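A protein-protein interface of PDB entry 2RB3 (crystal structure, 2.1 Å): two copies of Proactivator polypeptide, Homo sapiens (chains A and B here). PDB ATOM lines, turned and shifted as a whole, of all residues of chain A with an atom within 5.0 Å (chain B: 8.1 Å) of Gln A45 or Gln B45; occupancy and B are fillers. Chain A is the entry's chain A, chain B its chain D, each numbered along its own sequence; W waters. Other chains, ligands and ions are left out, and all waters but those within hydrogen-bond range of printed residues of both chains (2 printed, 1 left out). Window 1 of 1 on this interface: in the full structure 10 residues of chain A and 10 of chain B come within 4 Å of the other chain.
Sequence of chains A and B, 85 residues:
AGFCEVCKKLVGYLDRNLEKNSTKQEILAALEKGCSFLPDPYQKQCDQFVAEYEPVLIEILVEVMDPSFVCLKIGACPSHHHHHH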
ATOM      1  N   GLY A   2      -7.259  14.044   9.182  1.00  0.00           N
ATOM      2  CA  GLY A   2      -6.240  13.261   9.885  1.00  0.00           C
ATOM      3  C   GLY A   2      -5.046  12.880   9.017  1.00  0.00           C
ATOM      4  O   GLY A   2      -5.000  13.202   7.820  1.00  0.00           O
ATOM      5  N   PHE A   3      -4.092  12.178   9.632  1.00  0.00           N
ATOM      6  CA  PHE A   3      -2.841  11.773   8.982  1.00  0.00           C
ATOM      7  C   PHE A   3      -2.881  10.385   8.325  1.00  0.00           C
ATOM      8  O   PHE A   3      -1.861   9.925   7.810  1.00  0.00           O
ATOM      9  CB  PHE A   3      -1.682  11.780   9.988  1.00  0.00           C
ATOM     10  CG  PHE A   3      -1.217  13.146  10.397  1.00  0.00           C
ATOM     11  CD1 PHE A   3      -0.798  14.079   9.450  1.00  0.00           C
ATOM     12  CD2 PHE A   3      -1.155  13.487  11.753  1.00  0.00           C
ATOM     13  CE1 PHE A   3      -0.350  15.334   9.848  1.00  0.00           C
ATOM     14  CE2 PHE A   3      -0.715  14.742  12.155  1.00  0.00           C
ATOM     15  CZ  PHE A   3      -0.306  15.665  11.200  1.00  0.00           C
ATOM     16  N   VAL A   6      -1.982  10.205   4.295  1.00  0.00           N
ATOM     17  CA  VAL A   6      -0.599  10.623   4.061  1.00  0.00           C
ATOM     18  C   VAL A   6       0.389   9.592   4.636  1.00  0.00           C
ATOM     19  O   VAL A   6       1.398   9.271   4.001  1.00  0.00           O
ATOM     20  CB  VAL A   6      -0.335  12.087   4.573  1.00  0.00           C
ATOM     21  CG1 VAL A   6      -0.075  12.136   6.088  1.00  0.00           C
ATOM     22  CG2 VAL A   6       0.798  12.735   3.787  1.00  0.00           C
ATOM     23  N   PRO A  41       0.326  18.058  -3.615  1.00  0.00           N
ATOM     24  CA  PRO A  41      -0.684  18.463  -2.638  1.00  0.00           C
ATOM     25  C   PRO A  41      -0.421  17.970  -1.210  1.00  0.00           C
ATOM     26  O   PRO A  41      -0.897  18.595  -0.269  1.00  0.00           O
ATOM     27  CB  PRO A  41      -1.974  17.845  -3.194  1.00  0.00           C
ATOM     28  CG  PRO A  41      -1.752  17.822  -4.660  1.00  0.00           C
ATOM     29  CD  PRO A  41      -0.306  17.440  -4.800  1.00  0.00           C
ATOM     30  N   TYR A  42       0.340  16.879  -1.077  1.00  0.00           N
ATOM     31  CA  TYR A  42       0.611  16.214   0.211  1.00  0.00           C
ATOM     32  C   TYR A  42       1.833  16.727   0.970  1.00  0.00           C
ATOM     33  O   TYR A  42       2.004  16.401   2.147  1.00  0.00           O
ATOM     34  CB  TYR A  42       0.749  14.695   0.008  1.00  0.00           C
ATOM     35  CG  TYR A  42      -0.560  14.010  -0.274  1.00  0.00           C
ATOM     36  CD1 TYR A  42      -1.371  13.562   0.770  1.00  0.00           C
ATOM     37  CD2 TYR A  42      -1.008  13.831  -1.583  1.00  0.00           C
ATOM     38  CE1 TYR A  42      -2.593  12.944   0.516  1.00  0.00           C
ATOM     39  CE2 TYR A  42      -2.233  13.217  -1.846  1.00  0.00           C
ATOM     40  CZ  TYR A  42      -3.020  12.781  -0.790  1.00  0.00           C
ATOM     41  OH  TYR A  42      -4.226  12.161  -1.046  1.00  0.00           O
ATOM     42  N   GLN A  43       2.673  17.517   0.297  1.00  0.00           N
ATOM     43  CA  GLN A  43       3.981  17.931   0.827  1.00  0.00           C
ATOM     44  C   GLN A  43       3.994  18.410   2.282  1.00  0.00           C
ATOM     45  O   GLN A  43       4.641  17.782   3.114  1.00  0.00           O
ATOM     46  CB  GLN A  43       4.647  18.984  -0.067  1.00  0.00           C
ATOM     47  CG  GLN A  43       6.039  19.435   0.417  1.00  0.00           C
ATOM     48  CD  GLN A  43       7.132  18.415   0.153  1.00  0.00           C
ATOM     49  OE1 GLN A  43       7.747  17.871   1.083  1.00  0.00           O
ATOM     50  NE2 GLN A  43       7.386  18.152  -1.118  1.00  0.00           N
ATOM     51  N   LYS A  44       3.322  19.536   2.560  1.00  0.00           N
ATOM     52  CA  LYS A  44       3.388  20.183   3.874  1.00  0.00           C
ATOM     53  C   LYS A  44       2.654  19.385   4.955  1.00  0.00           C
ATOM     54  O   LYS A  44       3.044  19.430   6.123  1.00  0.00           O
ATOM     55  CB  LYS A  44       2.870  21.633   3.832  1.00  0.00           C
ATOM     56  CG  LYS A  44       3.645  22.592   2.927  1.00  0.00           C
ATOM     57  CD  LYS A  44       5.087  22.800   3.376  1.00  0.00           C
ATOM     58  CE  LYS A  44       5.759  23.890   2.525  1.00  0.00           C
ATOM     59  NZ  LYS A  44       7.232  23.944   2.765  1.00  0.00           N
ATOM     60  N   GLN A  45       1.596  18.676   4.566  1.00  0.00           N
ATOM     61  CA  GLN A  45       0.921  17.734   5.471  1.00  0.00           C
ATOM     62  C   GLN A  45       1.838  16.580   5.833  1.00  0.00           C
ATOM     63  O   GLN A  45       1.897  16.156   6.995  1.00  0.00           O
ATOM     64  CB  GLN A  45      -0.364  17.165   4.853  1.00  0.00           C
ATOM     65  CG  GLN A  45      -1.014  16.104   5.765  1.00  0.00           C
ATOM     66  CD  GLN A  45      -2.177  15.376   5.139  1.00  0.00           C
ATOM     67  OE1 GLN A  45      -2.137  14.985   3.973  1.00  0.00           O
ATOM     68  NE2 GLN A  45      -3.227  15.183   5.919  1.00  0.00           N
ATOM     69  N   CYS A  46       2.531  16.056   4.822  1.00  0.00           N
ATOM     70  CA  CYS A  46       3.501  14.975   5.027  1.00  0.00           C
ATOM     71  C   CYS A  46       4.672  15.428   5.903  1.00  0.00           C
ATOM     72  O   CYS A  46       5.086  14.678   6.796  1.00  0.00           O
ATOM     73  CB  CYS A  46       4.012  14.417   3.694  1.00  0.00           C
ATOM     74  SG  CYS A  46       5.111  12.999   3.857  1.00  0.00           S
ATOM     75  N   ASP A  47       5.197  16.636   5.660  1.00  0.00           N
ATOM     76  CA  ASP A  47       6.287  17.185   6.501  1.00  0.00           C
ATOM     77  C   ASP A  47       5.846  17.248   7.973  1.00  0.00           C
ATOM     78  O   ASP A  47       6.636  16.956   8.880  1.00  0.00           O
ATOM     79  CB  ASP A  47       6.689  18.595   6.082  1.00  0.00           C
ATOM     80  CG  ASP A  47       7.297  18.669   4.686  1.00  0.00           C
ATOM     81  OD1 ASP A  47       7.889  17.683   4.193  1.00  0.00           O
ATOM     82  OD2 ASP A  47       7.183  19.754   4.090  1.00  0.00           O
ATOM     83  N   GLN A  48       4.588  17.638   8.187  1.00  0.00           N
ATOM     84  CA  GLN A  48       4.013  17.746   9.534  1.00  0.00           C
ATOM     85  C   GLN A  48       3.840  16.368  10.161  1.00  0.00           C
ATOM     86  O   GLN A  48       4.249  16.147  11.298  1.00  0.00           O
ATOM     87  CB  GLN A  48       2.667  18.491   9.525  1.00  0.00           C
ATOM     88  CG  GLN A  48       2.152  18.806  10.947  1.00  0.00           C
ATOM     89  CD  GLN A  48       0.761  19.414  10.975  1.00  0.00           C
ATOM     90  OE1 GLN A  48       0.200  19.660  12.052  1.00  0.00           O
ATOM     91  NE2 GLN A  48       0.198  19.671   9.806  1.00  0.00           N
ATOM     92  N   PHE A  49       3.236  15.449   9.415  1.00  0.00           N
ATOM     93  CA  PHE A  49       3.133  14.062   9.853  1.00  0.00           C
ATOM     94  C   PHE A  49       4.493  13.487  10.281  1.00  0.00           C
ATOM     95  O   PHE A  49       4.610  12.886  11.350  1.00  0.00           O
ATOM     96  CB  PHE A  49       2.491  13.170   8.777  1.00  0.00           C
ATOM     97  CG  PHE A  49       2.656  11.707   9.050  1.00  0.00           C
ATOM     98  CD1 PHE A  49       1.977  11.107  10.115  1.00  0.00           C
ATOM     99  CD2 PHE A  49       3.514  10.931   8.278  1.00  0.00           C
ATOM    100  CE1 PHE A  49       2.157   9.748  10.395  1.00  0.00           C
ATOM    101  CE2 PHE A  49       3.695   9.568   8.553  1.00  0.00           C
ATOM    102  CZ  PHE A  49       3.025   8.985   9.618  1.00  0.00           C
ATOM    103  N   ALA B   1       2.380  23.724  16.954  1.00  0.00           N
ATOM    104  CA  ALA B   1       3.151  24.537  15.967  1.00  0.00           C
ATOM    105  C   ALA B   1       2.892  24.112  14.516  1.00  0.00           C
ATOM    106  O   ALA B   1       3.185  24.872  13.576  1.00  0.00           O
ATOM    107  CB  ALA B   1       4.642  24.467  16.286  1.00  0.00           C
ATOM    108  N   GLY B   2       2.335  22.907  14.347  1.00  0.00           N
ATOM    109  CA  GLY B   2       2.183  22.270  13.036  1.00  0.00           C
ATOM    110  C   GLY B   2       1.352  23.023  12.019  1.00  0.00           C
ATOM    111  O   GLY B   2       1.721  23.091  10.843  1.00  0.00           O
ATOM    112  N   PHE B   3       0.240  23.600  12.471  1.00  0.00           N
ATOM    113  CA  PHE B   3      -0.702  24.284  11.577  1.00  0.00           C
ATOM    114  C   PHE B   3      -0.501  25.799  11.452  1.00  0.00           C
ATOM    115  O   PHE B   3      -1.278  26.466  10.767  1.00  0.00           O
ATOM    116  CB  PHE B   3      -2.148  24.019  12.011  1.00  0.00           C
ATOM    117  CG  PHE B   3      -2.632  22.638  11.712  1.00  0.00           C
ATOM    118  CD1 PHE B   3      -2.565  22.121  10.417  1.00  0.00           C
ATOM    119  CD2 PHE B   3      -3.185  21.855  12.722  1.00  0.00           C
ATOM    120  CE1 PHE B   3      -3.025  20.842  10.138  1.00  0.00           C
ATOM    121  CE2 PHE B   3      -3.645  20.572  12.452  1.00  0.00           C
ATOM    122  CZ  PHE B   3      -3.566  20.066  11.154  1.00  0.00           C
ATOM    123  N   CYS B   4       0.531  26.338  12.095  1.00  0.00           N
ATOM    124  CA  CYS B   4       0.678  27.796  12.186  1.00  0.00           C
ATOM    125  C   CYS B   4       0.801  28.517  10.840  1.00  0.00           C
ATOM    126  O   CYS B   4       0.074  29.488  10.593  1.00  0.00           O
ATOM    127  CB  CYS B   4       1.821  28.198  13.129  1.00  0.00           C
ATOM    128  SG  CYS B   4       2.054  30.001  13.320  1.00  0.00           S
ATOM    129  N   GLU B   5       1.706  28.058   9.978  1.00  0.00           N
ATOM    130  CA  GLU B   5       1.907  28.727   8.683  1.00  0.00           C
ATOM    131  C   GLU B   5       0.746  28.554   7.703  1.00  0.00           C
ATOM    132  O   GLU B   5       0.433  29.473   6.940  1.00  0.00           O
ATOM    133  CB  GLU B   5       3.236  28.329   8.021  1.00  0.00           C
ATOM    134  CG  GLU B   5       3.638  29.257   6.855  1.00  0.00           C
ATOM    135  CD  GLU B   5       3.476  30.751   7.189  1.00  0.00           C
ATOM    136  OE1 GLU B   5       4.208  31.251   8.078  1.00  0.00           O
ATOM    137  OE2 GLU B   5       2.610  31.423   6.570  1.00  0.00           O
ATOM    138  N   VAL B   6       0.119  27.381   7.710  1.00  0.00           N
ATOM    139  CA  VAL B   6      -1.034  27.143   6.841  1.00  0.00           C
ATOM    140  C   VAL B   6      -2.258  27.959   7.300  1.00  0.00           C
ATOM    141  O   VAL B   6      -3.034  28.445   6.473  1.00  0.00           O
ATOM    142  CB  VAL B   6      -1.343  25.619   6.652  1.00  0.00           C
ATOM    143  CG1 VAL B   6      -2.001  25.001   7.895  1.00  0.00           C
ATOM    144  CG2 VAL B   6      -2.207  25.402   5.421  1.00  0.00           C
ATOM    145  N   CYS B   7      -2.403  28.119   8.615  1.00  0.00           N
ATOM    146  CA  CYS B   7      -3.472  28.925   9.193  1.00  0.00           C
ATOM    147  C   CYS B   7      -3.371  30.370   8.712  1.00  0.00           C
ATOM    148  O   CYS B   7      -4.352  30.935   8.251  1.00  0.00           O
ATOM    149  CB  CYS B   7      -3.414  28.872  10.723  1.00  0.00           C
ATOM    150  SG  CYS B   7      -4.679  29.858  11.560  1.00  0.00           S
ATOM    151  N   LYS B   9      -1.692  31.574   6.097  1.00  0.00           N
ATOM    152  CA  LYS B   9      -1.938  31.608   4.650  1.00  0.00           C
ATOM    153  C   LYS B   9      -3.423  31.537   4.300  1.00  0.00           C
ATOM    154  O   LYS B   9      -3.887  32.267   3.424  1.00  0.00           O
ATOM    155  CB  LYS B   9      -1.172  30.501   3.922  1.00  0.00           C
ATOM    156  CG  LYS B   9       0.251  30.875   3.595  1.00  0.00           C
ATOM    157  CD  LYS B   9       1.014  29.699   3.038  1.00  0.00           C
ATOM    158  CE  LYS B   9       2.419  30.106   2.649  1.00  0.00           C
ATOM    159  NZ  LYS B   9       2.425  30.908   1.394  1.00  0.00           N
ATOM    160  N   LEU B  10      -4.162  30.659   4.979  1.00  0.00           N
ATOM    161  CA  LEU B  10      -5.596  30.524   4.731  1.00  0.00           C
ATOM    162  C   LEU B  10      -6.412  31.743   5.201  1.00  0.00           C
ATOM    163  O   LEU B  10      -7.254  32.240   4.457  1.00  0.00           O
ATOM    164  CB  LEU B  10      -6.151  29.235   5.348  1.00  0.00           C
ATOM    165  CG  LEU B  10      -7.669  29.034   5.219  1.00  0.00           C
ATOM    166  CD1 LEU B  10      -8.069  28.686   3.797  1.00  0.00           C
ATOM    167  CD2 LEU B  10      -8.132  27.971   6.176  1.00  0.00           C
ATOM    168  N   CYS B  35      -8.841  26.617   0.733  1.00  0.00           N
ATOM    169  CA  CYS B  35      -7.682  25.739   0.622  1.00  0.00           C
ATOM    170  C   CYS B  35      -7.264  25.536  -0.835  1.00  0.00           C
ATOM    171  O   CYS B  35      -6.076  25.467  -1.118  1.00  0.00           O
ATOM    172  CB  CYS B  35      -7.923  24.408   1.332  1.00  0.00           C
ATOM    173  SG  CYS B  35      -8.077  24.537   3.151  1.00  0.00           S
ATOM    174  N   LEU B  38      -4.700  28.211  -2.117  1.00  0.00           N
ATOM    175  CA  LEU B  38      -3.326  28.203  -1.595  1.00  0.00           C
ATOM    176  C   LEU B  38      -2.385  27.435  -2.536  1.00  0.00           C
ATOM    177  O   LEU B  38      -2.851  26.636  -3.352  1.00  0.00           O
ATOM    178  CB  LEU B  38      -3.297  27.607  -0.177  1.00  0.00           C
ATOM    179  CG  LEU B  38      -3.302  28.549   1.033  1.00  0.00           C
ATOM    180  CD1 LEU B  38      -4.519  29.484   1.082  1.00  0.00           C
ATOM    181  CD2 LEU B  38      -3.189  27.752   2.332  1.00  0.00           C
ATOM    182  N   ASP B  40      -0.086  24.631  -4.164  1.00  0.00           N
ATOM    183  CA  ASP B  40      -0.282  23.178  -4.147  1.00  0.00           C
ATOM    184  C   ASP B  40       0.312  22.429  -2.937  1.00  0.00           C
ATOM    185  O   ASP B  40      -0.372  21.572  -2.375  1.00  0.00           O
ATOM    186  CB  ASP B  40       0.195  22.545  -5.457  1.00  0.00           C
ATOM    187  CG  ASP B  40      -0.835  22.658  -6.566  1.00  0.00           C
ATOM    188  OD1 ASP B  40      -1.550  23.688  -6.640  1.00  0.00           O
ATOM    189  OD2 ASP B  40      -0.934  21.704  -7.367  1.00  0.00           O
ATOM    190  N   PRO B  41       1.575  22.734  -2.537  1.00  0.00           N
ATOM    191  CA  PRO B  41       2.164  22.034  -1.371  1.00  0.00           C
ATOM    192  C   PRO B  41       1.348  22.080  -0.068  1.00  0.00           C
ATOM    193  O   PRO B  41       1.491  21.180   0.770  1.00  0.00           O
ATOM    194  CB  PRO B  41       3.506  22.744  -1.174  1.00  0.00           C
ATOM    195  CG  PRO B  41       3.858  23.261  -2.541  1.00  0.00           C
ATOM    196  CD  PRO B  41       2.542  23.670  -3.143  1.00  0.00           C
ATOM    197  N   TYR B  42       0.510  23.109   0.084  1.00  0.00           N
ATOM    198  CA  TYR B  42      -0.262  23.369   1.312  1.00  0.00           C
ATOM    199  C   TYR B  42      -1.672  22.765   1.339  1.00  0.00           C
ATOM    200  O   TYR B  42      -2.340  22.781   2.370  1.00  0.00           O
ATOM    201  CB  TYR B  42      -0.379  24.880   1.536  1.00  0.00           C
ATOM    202  CG  TYR B  42       0.881  25.518   2.058  1.00  0.00           C
ATOM    203  CD1 TYR B  42       1.094  25.657   3.427  1.00  0.00           C
ATOM    204  CD2 TYR B  42       1.860  25.986   1.184  1.00  0.00           C
ATOM    205  CE1 TYR B  42       2.249  26.247   3.910  1.00  0.00           C
ATOM    206  CE2 TYR B  42       3.022  26.568   1.658  1.00  0.00           C
ATOM    207  CZ  TYR B  42       3.206  26.690   3.023  1.00  0.00           C
ATOM    208  OH  TYR B  42       4.348  27.265   3.499  1.00  0.00           O
ATOM    209  N   GLN B  43      -2.123  22.252   0.204  1.00  0.00           N
ATOM    210  CA  GLN B  43      -3.515  21.838   0.025  1.00  0.00           C
ATOM    211  C   GLN B  43      -4.065  20.832   1.055  1.00  0.00           C
ATOM    212  O   GLN B  43      -4.984  21.167   1.797  1.00  0.00           O
ATOM    213  CB  GLN B  43      -3.719  21.352  -1.414  1.00  0.00           C
ATOM    214  CG  GLN B  43      -5.040  20.650  -1.684  1.00  0.00           C
ATOM    215  CD  GLN B  43      -5.215  20.336  -3.154  1.00  0.00           C
ATOM    216  OE1 GLN B  43      -5.277  19.170  -3.550  1.00  0.00           O
ATOM    217  NE2 GLN B  43      -5.274  21.384  -3.979  1.00  0.00           N
ATOM    218  N   LYS B  44      -3.508  19.617   1.090  1.00  0.00           N
ATOM    219  CA  LYS B  44      -3.973  18.555   1.995  1.00  0.00           C
ATOM    220  C   LYS B  44      -3.850  18.919   3.484  1.00  0.00           C
ATOM    221  O   LYS B  44      -4.736  18.591   4.275  1.00  0.00           O
ATOM    222  CB  LYS B  44      -3.268  17.221   1.709  1.00  0.00           C
ATOM    223  CG  LYS B  44      -3.600  16.584   0.356  1.00  0.00           C
ATOM    224  CD  LYS B  44      -5.082  16.257   0.209  1.00  0.00           C
ATOM    225  CE  LYS B  44      -5.381  15.741  -1.196  1.00  0.00           C
ATOM    226  NZ  LYS B  44      -6.710  15.079  -1.272  1.00  0.00           N
ATOM    227  N   GLN B  45      -2.750  19.584   3.847  1.00  0.00           N
ATOM    228  CA  GLN B  45      -2.579  20.166   5.182  1.00  0.00           C
ATOM    229  C   GLN B  45      -3.653  21.211   5.507  1.00  0.00           C
ATOM    230  O   GLN B  45      -4.199  21.225   6.617  1.00  0.00           O
ATOM    231  CB  GLN B  45      -1.195  20.807   5.330  1.00  0.00           C
ATOM    232  CG  GLN B  45      -0.962  21.413   6.719  1.00  0.00           C
ATOM    233  CD  GLN B  45       0.361  22.138   6.842  1.00  0.00           C
ATOM    234  OE1 GLN B  45       0.752  22.904   5.961  1.00  0.00           O
ATOM    235  NE2 GLN B  45       1.057  21.904   7.943  1.00  0.00           N
ATOM    236  N   CYS B  46      -3.943  22.086   4.547  1.00  0.00           N
ATOM    237  CA  CYS B  46      -5.005  23.094   4.730  1.00  0.00           C
ATOM    238  C   CYS B  46      -6.367  22.444   4.978  1.00  0.00           C
ATOM    239  O   CYS B  46      -7.096  22.863   5.877  1.00  0.00           O
ATOM    240  CB  CYS B  46      -5.089  24.050   3.539  1.00  0.00           C
ATOM    241  SG  CYS B  46      -6.318  25.374   3.756  1.00  0.00           S
ATOM    242  N   ASP B  47      -6.696  21.423   4.185  1.00  0.00           N
ATOM    243  CA  ASP B  47      -7.936  20.653   4.362  1.00  0.00           C
ATOM    244  C   ASP B  47      -8.059  20.090   5.780  1.00  0.00           C
ATOM    245  O   ASP B  47      -9.110  20.207   6.410  1.00  0.00           O
ATOM    246  CB  ASP B  47      -8.017  19.501   3.356  1.00  0.00           C
ATOM    247  CG  ASP B  47      -8.198  19.974   1.920  1.00  0.00           C
ATOM    248  OD1 ASP B  47      -8.604  21.134   1.701  1.00  0.00           O
ATOM    249  OD2 ASP B  47      -7.931  19.169   1.006  1.00  0.00           O
ATOM    250  N   GLN B  48      -6.982  19.481   6.264  1.00  0.00           N
ATOM    251  CA  GLN B  48      -6.941  18.907   7.610  1.00  0.00           C
ATOM    252  C   GLN B  48      -7.079  19.996   8.677  1.00  0.00           C
ATOM    253  O   GLN B  48      -7.772  19.806   9.677  1.00  0.00           O
ATOM    254  CB  GLN B  48      -5.668  18.072   7.820  1.00  0.00           C
ATOM    255  CG  GLN B  48      -5.603  17.350   9.192  1.00  0.00           C
ATOM    256  CD  GLN B  48      -4.253  16.685   9.474  1.00  0.00           C
ATOM    257  OE1 GLN B  48      -3.309  16.811   8.695  1.00  0.00           O
ATOM    258  NE2 GLN B  48      -4.160  15.977  10.602  1.00  0.00           N
ATOM    259  N   PHE B  49      -6.421  21.133   8.457  1.00  0.00           N
ATOM    260  CA  PHE B  49      -6.543  22.284   9.346  1.00  0.00           C
ATOM    261  C   PHE B  49      -7.986  22.798   9.439  1.00  0.00           C
ATOM    262  O   PHE B  49      -8.501  23.038  10.542  1.00  0.00           O
ATOM    263  CB  PHE B  49      -5.600  23.417   8.914  1.00  0.00           C
ATOM    264  CG  PHE B  49      -5.901  24.731   9.574  1.00  0.00           C
ATOM    265  CD1 PHE B  49      -5.703  24.898  10.948  1.00  0.00           C
ATOM    266  CD2 PHE B  49      -6.385  25.802   8.827  1.00  0.00           C
ATOM    267  CE1 PHE B  49      -5.989  26.115  11.563  1.00  0.00           C
ATOM    268  CE2 PHE B  49      -6.683  27.023   9.430  1.00  0.00           C
ATOM    269  CZ  PHE B  49      -6.490  27.176  10.802  1.00  0.00           C
ATOM    270  N   VAL B  50      -8.624  22.958   8.280  1.00  0.00           N
ATOM    271  CA  VAL B  50     -10.003  23.426   8.197  1.00  0.00           C
ATOM    272  C   VAL B  50     -10.965  22.461   8.874  1.00  0.00           C
ATOM    273  O   VAL B  50     -11.850  22.893   9.605  1.00  0.00           O
ATOM    274  CB  VAL B  50     -10.442  23.677   6.734  1.00  0.00           C
ATOM    275  CG1 VAL B  50     -11.964  23.902   6.643  1.00  0.00           C
ATOM    276  CG2 VAL B  50      -9.687  24.865   6.151  1.00  0.00           C
ATOM    277  N   ALA B  51     -10.776  21.165   8.636  1.00  0.00           N
ATOM    278  CA  ALA B  51     -11.608  20.124   9.241  1.00  0.00           C
ATOM    279  C   ALA B  51     -11.495  20.099  10.767  1.00  0.00           C
ATOM    280  O   ALA B  51     -12.491  19.883  11.468  1.00  0.00           O
ATOM    281  CB  ALA B  51     -11.245  18.756   8.654  1.00  0.00           C
ATOM    282  N   GLU B  52     -10.281  20.313  11.271  1.00  0.00           N
ATOM    283  CA  GLU B  52     -10.005  20.277  12.702  1.00  0.00           C
ATOM    284  C   GLU B  52     -10.518  21.542  13.402  1.00  0.00           C
ATOM    285  O   GLU B  52     -11.125  21.464  14.474  1.00  0.00           O
ATOM    286  CB  GLU B  52      -8.498  20.077  12.947  1.00  0.00           C
ATOM    287  CG  GLU B  52      -8.120  19.712  14.387  1.00  0.00           C
ATOM    288  CD  GLU B  52      -6.721  19.104  14.517  1.00  0.00           C
ATOM    289  OE1 GLU B  52      -6.350  18.234  13.698  1.00  0.00           O
ATOM    290  OE2 GLU B  52      -5.997  19.482  15.459  1.00  0.00           O
HETATM  291  O   HOH W   1      -1.341  18.431   8.158  1.00  0.00           O
HETATM  292  O   HOH W   2       4.438  21.459   7.200  1.00  0.00           O
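The backbone NH (N) of Lys B44 is in hydrogen-bond range of the backbone carbonyl oxygen (O) of Pro A41 (3.1 Å). N of Lys A44 sits at hydrogen-bond distance from O of Pro B41 (3.0 Å). NE2 of Gln A45 sits at hydrogen-bond distance from OE1 of Gln B48 (3.2 Å). The side-chain amide nitrogen (NE2) of Gln B45 sits close to the side-chain amide nitrogen (NE2) of Gln A48 (3.0 Å).
The backbone carbonyl oxygen (O) of Gly A2 is in hydrogen-bond range of the side-chain amide nitrogen (NE2) of Gln A45 (3.3 Å). The side-chain amide oxygen (OE1) of Gln A43 sits close to the side-chain carboxylate (OD1) of Asp A47, at 3.1 Å. The side-chain amide nitrogen of Gln B45 lies within hydrogen-bond range of the backbone carbonyl oxygen of Gly B2 (3.2 Å). The side-chain sulfur of Cys B46 is disulfide-bonded to the side-chain sulfur of Cys B35 (2.0 Å).
Among the printed residues, merely in contact across the chains: Gly A2 with Gln B48 (3.5 Å), Phe A3 with Gln B48 (3.5 Å), Pro A41 with Asp B40 (3.1 Å), Pro A41 with Pro B41 (3.7 Å), Pro A41 with Gln B43 (3.6 Å), Tyr A42 with Lys B44 (3.8 Å), Gln A43 with Pro B41 (3.9 Å), Lys A44 with Tyr B42 (3.8 Å), Lys A44 with Gln B45 (3.3 Å), Gln A45 with Lys B44 (3.4 Å), Gln A45 with Gln B45 (3.5 Å), Gln A48 with Gly B2 (3.4 Å) and Gln A48 with Phe B3 (3.4 Å).
Gln A45 touches just these residues of chain B: Lys B44 (3.4 Å), Gln B45 (3.5 Å) and Gln B48 (3.2 Å). Of chain A, only Lys A44 (3.3 Å), Gln A45 (3.5 Å) and Gln A48 (3.0 Å) come within 4 Å of Gln B45. Of the printed residues of chain B, Gly A2 touches Gln B48. Printed residues of chain A within 4 Å of Gln B48: Gly A2 (3.5 Å), Phe A3 (3.5 Å) and Gln A45 (3.2 Å). Of the printed residues of chain B, Phe A3 touches Gln B48. The nearest residue of chain B that does not touch Gln A45 is Pro B41 (4.5 Å). The nearest residue of chain A that does not touch Gln B45 is Pro A41 (4.6 Å).
Printed residues of chain B that touch a printed residue of chain A: Gly B2, Phe B3, Asp B40, Pro B41, Tyr B42, Gln B43, Lys B44, Gln B45 and Gln B48. Hydrophobic or aromatic side chains of chain B that line the printed part of chain A: Phe B3 and Tyr B42. Along chain B the printed residues that touch a printed residue of chain A span positions 2 to 48. Among the printed residues, no Asp or Glu carboxylate lies within 4 Å of a Lys or Arg side-chain nitrogen of the other chain.
Gly A2 touches Gln B48, and with the chains exchanged Gln A48 touches Gly B2. Tyr A42 touches Lys B44, and with the chains exchanged Lys A44 touches Tyr B42. Lys A44 touches Gln B45, and with the chains exchanged Gln A45 touches Lys B44. Gln B45 touches its own counterpart, Gln A45. Positions printed for both chains: 2, 3, 6, 41, 42, 43, 44, 45, 46, 47, 48 and 49. Of the 17 pairs that touch across the chains among the printed residues, 16 have their exchanged pair printed and touching as well.
Water W1 lies within hydrogen-bond range of the side-chain amide nitrogen (NE2) of Gln A48 (2.6 Å) and the side-chain amide oxygen (OE1) of Gln B48 (2.6 Å). Water W2 lies within hydrogen-bond range of O of Lys A44 (2.7 Å) and NE2 of Gln B45 (3.5 Å).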
